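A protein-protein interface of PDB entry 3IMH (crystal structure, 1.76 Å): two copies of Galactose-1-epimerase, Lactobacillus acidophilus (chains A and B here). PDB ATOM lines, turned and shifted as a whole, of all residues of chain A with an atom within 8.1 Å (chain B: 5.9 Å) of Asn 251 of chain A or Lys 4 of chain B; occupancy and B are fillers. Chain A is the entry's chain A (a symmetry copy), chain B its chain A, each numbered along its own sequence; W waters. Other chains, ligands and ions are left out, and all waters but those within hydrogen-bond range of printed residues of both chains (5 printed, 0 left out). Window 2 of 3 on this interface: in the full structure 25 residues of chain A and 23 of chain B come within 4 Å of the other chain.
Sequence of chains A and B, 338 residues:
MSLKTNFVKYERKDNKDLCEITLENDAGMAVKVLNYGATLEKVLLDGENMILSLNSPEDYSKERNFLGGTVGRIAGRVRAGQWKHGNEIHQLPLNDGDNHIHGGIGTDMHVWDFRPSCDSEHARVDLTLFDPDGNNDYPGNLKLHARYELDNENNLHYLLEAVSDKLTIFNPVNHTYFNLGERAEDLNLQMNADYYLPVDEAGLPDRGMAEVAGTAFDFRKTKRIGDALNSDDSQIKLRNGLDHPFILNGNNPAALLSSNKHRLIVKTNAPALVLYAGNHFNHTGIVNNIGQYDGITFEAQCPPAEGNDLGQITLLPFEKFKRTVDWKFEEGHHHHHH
Water W3 bridges ND2 of Asn 6 of chain B (2.7 Å) and OD2 of Asp 194 of chain A (3.1 Å).
Water W5 lies within hydrogen-bond range of O of Gly 250 of chain A (2.7 Å), OD1 of Asn 252 of chain A (2.8 Å) and N of Cys 118 of chain B (3.1 Å).
Water W1 lies within hydrogen-bond range of ND2 of Asn 251 of chain A (2.8 Å), O of Leu 3 of chain B (2.8 Å) and SG of Cys 118 of chain B (3.5 Å).
Water W4 lies within hydrogen-bond range of the side-chain carboxylate of Asp 194 of chain A (3.1 Å) and the side-chain amide nitrogen of Asn 6 of chain B (3.3 Å).
Water W2 lies within hydrogen-bond range of the backbone carbonyl oxygen (O) of Cys 118 of chain B (3.1 Å) and the side-chain amide oxygen (OD1) of Asn 252 of chain A (3.5 Å).
Of the printed residues of chain B, Leu 248 of chain A touches Pro 116.
Of the printed residues of chain A, Asn 6 of chain B touches Asp 194 (2.6 Å) and Asn 249 (3.5 Å).
Printed residues of chain A within 4 Å of Ser 117 of chain B: Gly 250 (3.6 Å).
Printed residues of chain A within 4 Å of Cys 118 of chain B: Gly 250, Asn 251 and Asn 252.
The nearest printed residue of chain B that does not touch Asn 252 of chain A is Ser 117 of chain B (6.0 Å).
The side-chain sulfur (SG) of Cys 118 of chain B lies within hydrogen-bond range of the backbone carbonyl oxygen (O) of Leu 3 of chain B.
O of Lys 4 of chain B is in hydrogen-bond range of N of Glu 24 of chain B (2.9 Å).
The backbone NH (N) of Thr 22 of chain B sits at hydrogen-bond distance from the backbone carbonyl oxygen (O) of Asn 6 of chain B (2.7 Å).
The backbone carbonyl oxygen of Asn 192 of chain A lies within hydrogen-bond range of the backbone NH of Asn 249 of chain A, 2.9 Å away.
The side-chain amide nitrogen (ND2) of Asn 192 of chain A lies within hydrogen-bond range of the backbone carbonyl oxygen (O) of Asn 251 of chain A (3.4 Å).
The side-chain amide nitrogen (ND2) of Asn 249 of chain A is in hydrogen-bond range of the side-chain carboxylate (OD1) of Asp 194 of chain A.
Leu 248 of chain A touches Pro 116 of chain B.
Asn 249 of chain A touches Asn 6 of chain B.
Pro 116 of chain B touches Asn 249 of chain A (CG to O, 3.3 Å).
Gly 250 of chain A touches Thr 5 of chain B.
Pro 116 of chain B touches Gly 250 of chain A (O to CA, 3.4 Å).
Gly 250 of chain A touches Ser 117 of chain B (O to CA, 3.6 Å).
Lys 4 of chain B touches Asn 251 of chain A (CB to ND2, 3.4 Å).
Asn 251 of chain A touches Cys 118 of chain B (ND2 to SG, 3.9 Å).
The backbone carbonyl oxygen (O) of Asn 249 of chain A lies within hydrogen-bond range of the side-chain hydroxyl (OG1) of Thr 5 of chain B.
O of Thr 5 of chain B lies close to OD1 of Asn 251 of chain A, at 2.8 Å.
The side-chain carboxylate (OD2) of Asp 194 of chain A is in hydrogen-bond range of the side-chain amide nitrogen (ND2) of Asn 6 of chain B, 2.6 Å away.
N of Cys 118 of chain B sits at hydrogen-bond distance from O of Gly 250 of chain A, 3.5 Å away.
ND2 of Asn 252 of chain A lies within hydrogen-bond range of O of Cys 118 of chain B.
No position is printed for both chains.
Printed residues of chain B that touch a printed residue of chain A: Lys 4, Thr 5, Asn 6, Pro 116, Ser 117 and Cys 118.
Of the 15 printed residues of chain A, 6 touch a printed residue of chain B.
Printed residues of chain A that touch a printed residue of chain B: Asp 194, Leu 248, Asn 249, Gly 250, Asn 251 and Asn 252.
Among the printed residues, 13 pairs touch across the chains.
Among the printed residues, no Asp or Glu carboxylate lies within 4 Å of a Lys or Arg side-chain nitrogen of the other chain.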
ATOM      1  N   GLN A 190      20.520  13.226 -13.966  1.00  0.00           N
ATOM      2  CA  GLN A 190      19.931  12.820 -12.689  1.00  0.00           C
ATOM      3  C   GLN A 190      21.056  12.943 -11.675  1.00  0.00           C
ATOM      4  O   GLN A 190      22.190  12.551 -11.956  1.00  0.00           O
ATOM      5  CB  GLN A 190      19.397  11.385 -12.737  1.00  0.00           C
ATOM      6  CG  GLN A 190      18.513  10.997 -11.521  1.00  0.00           C
ATOM      7  CD  GLN A 190      19.322  10.463 -10.358  1.00  0.00           C
ATOM      8  OE1 GLN A 190      20.375   9.843 -10.558  1.00  0.00           O
ATOM      9  NE2 GLN A 190      18.852  10.708  -9.136  1.00  0.00           N
ATOM     10  N   MET A 191      20.738  13.495 -10.508  1.00  0.00           N
ATOM     11  CA  MET A 191      21.761  13.717  -9.476  1.00  0.00           C
ATOM     12  C   MET A 191      21.191  13.439  -8.102  1.00  0.00           C
ATOM     13  O   MET A 191      20.131  13.968  -7.734  1.00  0.00           O
ATOM     14  CB  MET A 191      22.312  15.151  -9.586  1.00  0.00           C
ATOM     15  CG  MET A 191      23.445  15.530  -8.608  1.00  0.00           C
ATOM     16  SD  MET A 191      24.290  17.092  -9.069  1.00  0.00           S
ATOM     17  CE  MET A 191      22.849  18.082  -9.568  1.00  0.00           C
ATOM     18  N   ASN A 192      21.915  12.623  -7.334  1.00  0.00           N
ATOM     19  CA  ASN A 192      21.475  12.231  -6.004  1.00  0.00           C
ATOM     20  C   ASN A 192      21.879  13.282  -4.976  1.00  0.00           C
ATOM     21  O   ASN A 192      22.793  13.073  -4.180  1.00  0.00           O
ATOM     22  CB  ASN A 192      21.994  10.834  -5.656  1.00  0.00           C
ATOM     23  CG  ASN A 192      21.185   9.745  -6.341  1.00  0.00           C
ATOM     24  OD1 ASN A 192      19.968   9.873  -6.468  1.00  0.00           O
ATOM     25  ND2 ASN A 192      21.846   8.690  -6.798  1.00  0.00           N
ATOM     26  N   ALA A 193      21.192  14.420  -5.045  1.00  0.00           N
ATOM     27  CA  ALA A 193      21.400  15.556  -4.156  1.00  0.00           C
ATOM     28  C   ALA A 193      20.039  16.176  -3.927  1.00  0.00           C
ATOM     29  O   ALA A 193      19.343  16.513  -4.889  1.00  0.00           O
ATOM     30  CB  ALA A 193      22.350  16.584  -4.788  1.00  0.00           C
ATOM     31  N   ASP A 194      19.665  16.324  -2.658  1.00  0.00           N
ATOM     32  CA  ASP A 194      18.362  16.901  -2.279  1.00  0.00           C
ATOM     33  C   ASP A 194      18.491  18.373  -1.914  1.00  0.00           C
ATOM     34  O   ASP A 194      17.475  19.068  -1.742  1.00  0.00           O
ATOM     35  CB  ASP A 194      17.769  16.160  -1.085  1.00  0.00           C
ATOM     36  CG  ASP A 194      17.536  14.694  -1.370  1.00  0.00           C
ATOM     37  OD1 ASP A 194      17.279  14.340  -2.534  1.00  0.00           O
ATOM     38  OD2 ASP A 194      17.624  13.892  -0.433  1.00  0.00           O
ATOM     39  N   LEU A 248      25.584  16.185  -1.856  1.00  0.00           N
ATOM     40  CA  LEU A 248      25.188  14.807  -2.179  1.00  0.00           C
ATOM     41  C   LEU A 248      24.466  14.092  -1.025  1.00  0.00           C
ATOM     42  O   LEU A 248      24.804  14.294   0.146  1.00  0.00           O
ATOM     43  CB  LEU A 248      26.415  14.001  -2.621  1.00  0.00           C
ATOM     44  CG  LEU A 248      27.135  14.556  -3.868  1.00  0.00           C
ATOM     45  CD1 LEU A 248      28.427  13.780  -4.129  1.00  0.00           C
ATOM     46  CD2 LEU A 248      26.206  14.525  -5.105  1.00  0.00           C
ATOM     47  N   ASN A 249      23.475  13.265  -1.360  1.00  0.00           N
ATOM     48  CA  ASN A 249      22.693  12.579  -0.313  1.00  0.00           C
ATOM     49  C   ASN A 249      23.266  11.230   0.103  1.00  0.00           C
ATOM     50  O   ASN A 249      22.773  10.608   1.053  1.00  0.00           O
ATOM     51  CB  ASN A 249      21.181  12.482  -0.662  1.00  0.00           C
ATOM     52  CG  ASN A 249      20.878  11.580  -1.880  1.00  0.00           C
ATOM     53  OD1 ASN A 249      21.601  10.646  -2.211  1.00  0.00           O
ATOM     54  ND2 ASN A 249      19.763  11.878  -2.542  1.00  0.00           N
ATOM     55  N   GLY A 250      24.290  10.781  -0.630  1.00  0.00           N
ATOM     56  CA  GLY A 250      25.001   9.549  -0.308  1.00  0.00           C
ATOM     57  C   GLY A 250      24.618   8.326  -1.124  1.00  0.00           C
ATOM     58  O   GLY A 250      25.351   7.327  -1.132  1.00  0.00           O
ATOM     59  N   ASN A 251      23.489   8.384  -1.826  1.00  0.00           N
ATOM     60  CA  ASN A 251      23.111   7.271  -2.713  1.00  0.00           C
ATOM     61  C   ASN A 251      23.866   7.317  -4.034  1.00  0.00           C
ATOM     62  O   ASN A 251      24.285   8.385  -4.473  1.00  0.00           O
ATOM     63  CB  ASN A 251      21.601   7.241  -2.930  1.00  0.00           C
ATOM     64  CG  ASN A 251      20.851   7.198  -1.626  1.00  0.00           C
ATOM     65  OD1 ASN A 251      20.106   8.124  -1.281  1.00  0.00           O
ATOM     66  ND2 ASN A 251      21.080   6.143  -0.867  1.00  0.00           N
ATOM     67  N   ASN A 252      24.057   6.147  -4.635  1.00  0.00           N
ATOM     68  CA  ASN A 252      24.907   6.000  -5.816  1.00  0.00           C
ATOM     69  C   ASN A 252      24.097   5.992  -7.105  1.00  0.00           C
ATOM     70  O   ASN A 252      22.971   5.480  -7.114  1.00  0.00           O
ATOM     71  CB  ASN A 252      25.702   4.701  -5.731  1.00  0.00           C
ATOM     72  CG  ASN A 252      26.573   4.641  -4.506  1.00  0.00           C
ATOM     73  OD1 ASN A 252      27.425   5.500  -4.303  1.00  0.00           O
ATOM     74  ND2 ASN A 252      26.343   3.635  -3.668  1.00  0.00           N
ATOM     75  N   PRO A 253      24.652   6.566  -8.193  1.00  0.00           N
ATOM     76  CA  PRO A 253      25.896   7.343  -8.275  1.00  0.00           C
ATOM     77  C   PRO A 253      25.646   8.780  -7.857  1.00  0.00           C
ATOM     78  O   PRO A 253      24.493   9.166  -7.601  1.00  0.00           O
ATOM     79  CB  PRO A 253      26.233   7.283  -9.763  1.00  0.00           C
ATOM     80  CG  PRO A 253      24.880   7.296 -10.433  1.00  0.00           C
ATOM     81  CD  PRO A 253      23.991   6.457  -9.515  1.00  0.00           C
ATOM     82  N   ALA A 254      26.713   9.563  -7.755  1.00  0.00           N
ATOM     83  CA  ALA A 254      26.570  10.981  -7.438  1.00  0.00           C
ATOM     84  C   ALA A 254      25.770  11.701  -8.536  1.00  0.00           C
ATOM     85  O   ALA A 254      24.861  12.467  -8.237  1.00  0.00           O
ATOM     86  CB  ALA A 254      27.936  11.637  -7.249  1.00  0.00           C
ATOM     87  N   ALA A 255      26.085  11.403  -9.794  1.00  0.00           N
ATOM     88  CA  ALA A 255      25.408  12.029 -10.939  1.00  0.00           C
ATOM     89  C   ALA A 255      25.396  11.044 -12.099  1.00  0.00           C
ATOM     90  O   ALA A 255      26.299  10.209 -12.229  1.00  0.00           O
ATOM     91  CB  ALA A 255      26.121  13.324 -11.344  1.00  0.00           C
ATOM     92  N   VAL A 266      28.998   9.308 -12.611  1.00  0.00           N
ATOM     93  CA  VAL A 266      29.980  10.033 -11.790  1.00  0.00           C
ATOM     94  C   VAL A 266      29.914   9.543 -10.346  1.00  0.00           C
ATOM     95  O   VAL A 266      28.847   9.557  -9.727  1.00  0.00           O
ATOM     96  CB  VAL A 266      29.719  11.558 -11.785  1.00  0.00           C
ATOM     97  CG1 VAL A 266      30.844  12.298 -11.044  1.00  0.00           C
ATOM     98  CG2 VAL A 266      29.556  12.105 -13.219  1.00  0.00           C
ATOM     99  N   LYS A 267      31.062   9.116  -9.821  1.00  0.00           N
ATOM    100  CA  LYS A 267      31.181   8.758  -8.412  1.00  0.00           C
ATOM    101  C   LYS A 267      32.344   9.535  -7.800  1.00  0.00           C
ATOM    102  O   LYS A 267      33.282   9.905  -8.501  1.00  0.00           O
ATOM    103  CB  LYS A 267      31.411   7.262  -8.259  1.00  0.00           C
ATOM    104  CG  LYS A 267      30.181   6.441  -8.644  1.00  0.00           C
ATOM    105  CD  LYS A 267      30.463   4.977  -8.447  1.00  0.00           C
ATOM    106  CE  LYS A 267      29.338   4.144  -8.998  1.00  0.00           C
ATOM    107  NZ  LYS A 267      29.618   2.685  -8.847  1.00  0.00           N
ATOM    108  N   SER B   2      17.377  -1.728  -0.305  1.00  0.00           N
ATOM    109  CA  SER B   2      18.825  -1.421  -0.477  1.00  0.00           C
ATOM    110  C   SER B   2      19.358  -0.698   0.754  1.00  0.00           C
ATOM    111  O   SER B   2      18.607  -0.026   1.460  1.00  0.00           O
ATOM    112  CB  SER B   2      19.040  -0.537  -1.712  1.00  0.00           C
ATOM    113  OG  SER B   2      18.761  -1.246  -2.909  1.00  0.00           O
ATOM    114  N   LEU B   3      20.653  -0.847   1.008  1.00  0.00           N
ATOM    115  CA  LEU B   3      21.334   0.022   1.951  1.00  0.00           C
ATOM    116  C   LEU B   3      21.303   1.415   1.343  1.00  0.00           C
ATOM    117  O   LEU B   3      21.620   1.588   0.163  1.00  0.00           O
ATOM    118  CB  LEU B   3      22.775  -0.446   2.153  1.00  0.00           C
ATOM    119  CG  LEU B   3      22.815  -1.758   2.931  1.00  0.00           C
ATOM    120  CD1 LEU B   3      23.778  -2.742   2.298  1.00  0.00           C
ATOM    121  CD2 LEU B   3      23.163  -1.458   4.382  1.00  0.00           C
ATOM    122  N   LYS B   4      20.880   2.397   2.138  1.00  0.00           N
ATOM    123  CA  LYS B   4      20.664   3.747   1.628  1.00  0.00           C
ATOM    124  C   LYS B   4      20.841   4.773   2.732  1.00  0.00           C
ATOM    125  O   LYS B   4      20.824   4.436   3.916  1.00  0.00           O
ATOM    126  CB  LYS B   4      19.275   3.882   0.995  1.00  0.00           C
ATOM    127  CG  LYS B   4      18.114   3.712   1.951  1.00  0.00           C
ATOM    128  CD  LYS B   4      16.788   3.661   1.190  1.00  0.00           C
ATOM    129  CE  LYS B   4      15.653   3.238   2.108  1.00  0.00           C
ATOM    130  NZ  LYS B   4      14.338   3.155   1.411  1.00  0.00           N
ATOM    131  N   THR B   5      21.062   6.015   2.320  1.00  0.00           N
ATOM    132  CA  THR B   5      21.270   7.116   3.247  1.00  0.00           C
ATOM    133  C   THR B   5      20.478   8.294   2.742  1.00  0.00           C
ATOM    134  O   THR B   5      20.167   8.378   1.554  1.00  0.00           O
ATOM    135  CB  THR B   5      22.767   7.567   3.293  1.00  0.00           C
ATOM    136  OG1 THR B   5      23.186   7.955   1.979  1.00  0.00           O
ATOM    137  CG2 THR B   5      23.688   6.451   3.785  1.00  0.00           C
ATOM    138  N   ASN B   6      20.162   9.214   3.641  1.00  0.00           N
ATOM    139  CA  ASN B   6      19.660  10.519   3.245  1.00  0.00           C
ATOM    140  C   ASN B   6      19.771  11.408   4.459  1.00  0.00           C
ATOM    141  O   ASN B   6      20.123  10.940   5.548  1.00  0.00           O
ATOM    142  CB  ASN B   6      18.213  10.461   2.731  1.00  0.00           C
ATOM    143  CG  ASN B   6      17.969  11.404   1.535  1.00  0.00           C
ATOM    144  OD1 ASN B   6      17.280  11.043   0.582  1.00  0.00           O
ATOM    145  ND2 ASN B   6      18.541  12.610   1.585  1.00  0.00           N
ATOM    146  N   THR B  22      19.827   9.832   8.047  1.00  0.00           N
ATOM    147  CA  THR B  22      19.241   8.507   8.256  1.00  0.00           C
ATOM    148  C   THR B  22      20.007   7.455   7.461  1.00  0.00           C
ATOM    149  O   THR B  22      20.234   7.624   6.258  1.00  0.00           O
ATOM    150  CB  THR B  22      17.722   8.466   7.889  1.00  0.00           C
ATOM    151  OG1 THR B  22      17.025   9.434   8.674  1.00  0.00           O
ATOM    152  CG2 THR B  22      17.121   7.094   8.213  1.00  0.00           C
ATOM    153  N   LEU B  23      20.426   6.394   8.147  1.00  0.00           N
ATOM    154  CA  LEU B  23      21.028   5.217   7.514  1.00  0.00           C
ATOM    155  C   LEU B  23      20.007   4.097   7.585  1.00  0.00           C
ATOM    156  O   LEU B  23      19.432   3.859   8.646  1.00  0.00           O
ATOM    157  CB  LEU B  23      22.294   4.774   8.261  1.00  0.00           C
ATOM    158  CG  LEU B  23      23.274   5.854   8.740  1.00  0.00           C
ATOM    159  CD1 LEU B  23      24.399   5.204   9.541  1.00  0.00           C
ATOM    160  CD2 LEU B  23      23.835   6.623   7.549  1.00  0.00           C
ATOM    161  N   GLU B  24      19.772   3.417   6.469  1.00  0.00           N
ATOM    162  CA  GLU B  24      18.814   2.287   6.462  1.00  0.00           C
ATOM    163  C   GLU B  24      19.407   1.056   5.809  1.00  0.00           C
ATOM    164  O   GLU B  24      20.228   1.159   4.899  1.00  0.00           O
ATOM    165  CB  GLU B  24      17.521   2.668   5.729  1.00  0.00           C
ATOM    166  CG  GLU B  24      16.728   3.775   6.406  1.00  0.00           C
ATOM    167  CD  GLU B  24      15.500   4.196   5.618  1.00  0.00           C
ATOM    168  OE1 GLU B  24      15.567   5.219   4.902  1.00  0.00           O
ATOM    169  OE2 GLU B  24      14.474   3.498   5.714  1.00  0.00           O
ATOM    170  N   ASN B  25      18.979  -0.117   6.268  1.00  0.00           N
ATOM    171  CA  ASN B  25      19.443  -1.356   5.679  1.00  0.00           C
ATOM    172  C   ASN B  25      18.252  -2.182   5.178  1.00  0.00           C
ATOM    173  O   ASN B  25      17.119  -1.691   5.146  1.00  0.00           O
ATOM    174  CB  ASN B  25      20.355  -2.126   6.661  1.00  0.00           C
ATOM    175  CG  ASN B  25      19.619  -2.672   7.889  1.00  0.00           C
ATOM    176  OD1 ASN B  25      18.390  -2.628   7.983  1.00  0.00           O
ATOM    177  ND2 ASN B  25      20.389  -3.208   8.834  1.00  0.00           N
ATOM    178  N   PRO B 116      27.404  11.506   3.909  1.00  0.00           N
ATOM    179  CA  PRO B 116      26.844  10.161   3.849  1.00  0.00           C
ATOM    180  C   PRO B 116      27.400   9.397   2.642  1.00  0.00           C
ATOM    181  O   PRO B 116      27.769  10.015   1.632  1.00  0.00           O
ATOM    182  CB  PRO B 116      25.339  10.425   3.663  1.00  0.00           C
ATOM    183  CG  PRO B 116      25.289  11.731   2.905  1.00  0.00           C
ATOM    184  CD  PRO B 116      26.481  12.536   3.375  1.00  0.00           C
ATOM    185  N   SER B 117      27.453   8.069   2.740  1.00  0.00           N
ATOM    186  CA  SER B 117      27.756   7.235   1.577  1.00  0.00           C
ATOM    187  C   SER B 117      27.241   5.835   1.814  1.00  0.00           C
ATOM    188  O   SER B 117      26.906   5.452   2.947  1.00  0.00           O
ATOM    189  CB  SER B 117      29.264   7.191   1.275  1.00  0.00           C
ATOM    190  OG  SER B 117      30.000   6.659   2.365  1.00  0.00           O
ATOM    191  N   CYS B 118      27.165   5.065   0.741  1.00  0.00           N
ATOM    192  CA  CYS B 118      26.796   3.675   0.895  1.00  0.00           C
ATOM    193  C   CYS B 118      27.381   2.821  -0.221  1.00  0.00           C
ATOM    194  O   CYS B 118      27.890   3.333  -1.233  1.00  0.00           O
ATOM    195  CB  CYS B 118      25.281   3.506   1.003  1.00  0.00           C
ATOM    196  SG  CYS B 118      24.374   4.023  -0.443  1.00  0.00           S
ATOM    197  N   HIS B 122      27.336  -1.636   3.202  1.00  0.00           N
ATOM    198  CA  HIS B 122      27.155  -0.640   4.285  1.00  0.00           C
ATOM    199  C   HIS B 122      26.429   0.630   3.892  1.00  0.00           C
ATOM    200  O   HIS B 122      26.498   1.053   2.748  1.00  0.00           O
ATOM    201  CB  HIS B 122      28.512  -0.200   4.842  1.00  0.00           C
ATOM    202  CG  HIS B 122      29.352  -1.328   5.343  1.00  0.00           C
ATOM    203  ND1 HIS B 122      30.359  -1.890   4.589  1.00  0.00           N
ATOM    204  CD2 HIS B 122      29.327  -2.009   6.512  1.00  0.00           C
ATOM    205  CE1 HIS B 122      30.927  -2.861   5.278  1.00  0.00           C
ATOM    206  NE2 HIS B 122      30.319  -2.957   6.446  1.00  0.00           N
ATOM    207  N   ALA B 123      25.750   1.238   4.868  1.00  0.00           N
ATOM    208  CA  ALA B 123      25.266   2.615   4.764  1.00  0.00           C
ATOM    209  C   ALA B 123      25.942   3.355   5.915  1.00  0.00           C
ATOM    210  O   ALA B 123      25.940   2.873   7.063  1.00  0.00           O
ATOM    211  CB  ALA B 123      23.748   2.686   4.903  1.00  0.00           C
HETATM  212  O   HOH W   1      21.212   3.555  -1.819  1.00  0.00           O
HETATM  213  O   HOH W   2      30.343   4.380  -2.842  1.00  0.00           O
HETATM  214  O   HOH W   3      19.692  14.997   1.574  1.00  0.00           O
HETATM  215  O   HOH W   4      16.073  14.765   2.046  1.00  0.00           O
HETATM  216  O   HOH W   5      27.923   6.649  -1.801  1.00  0.00           O
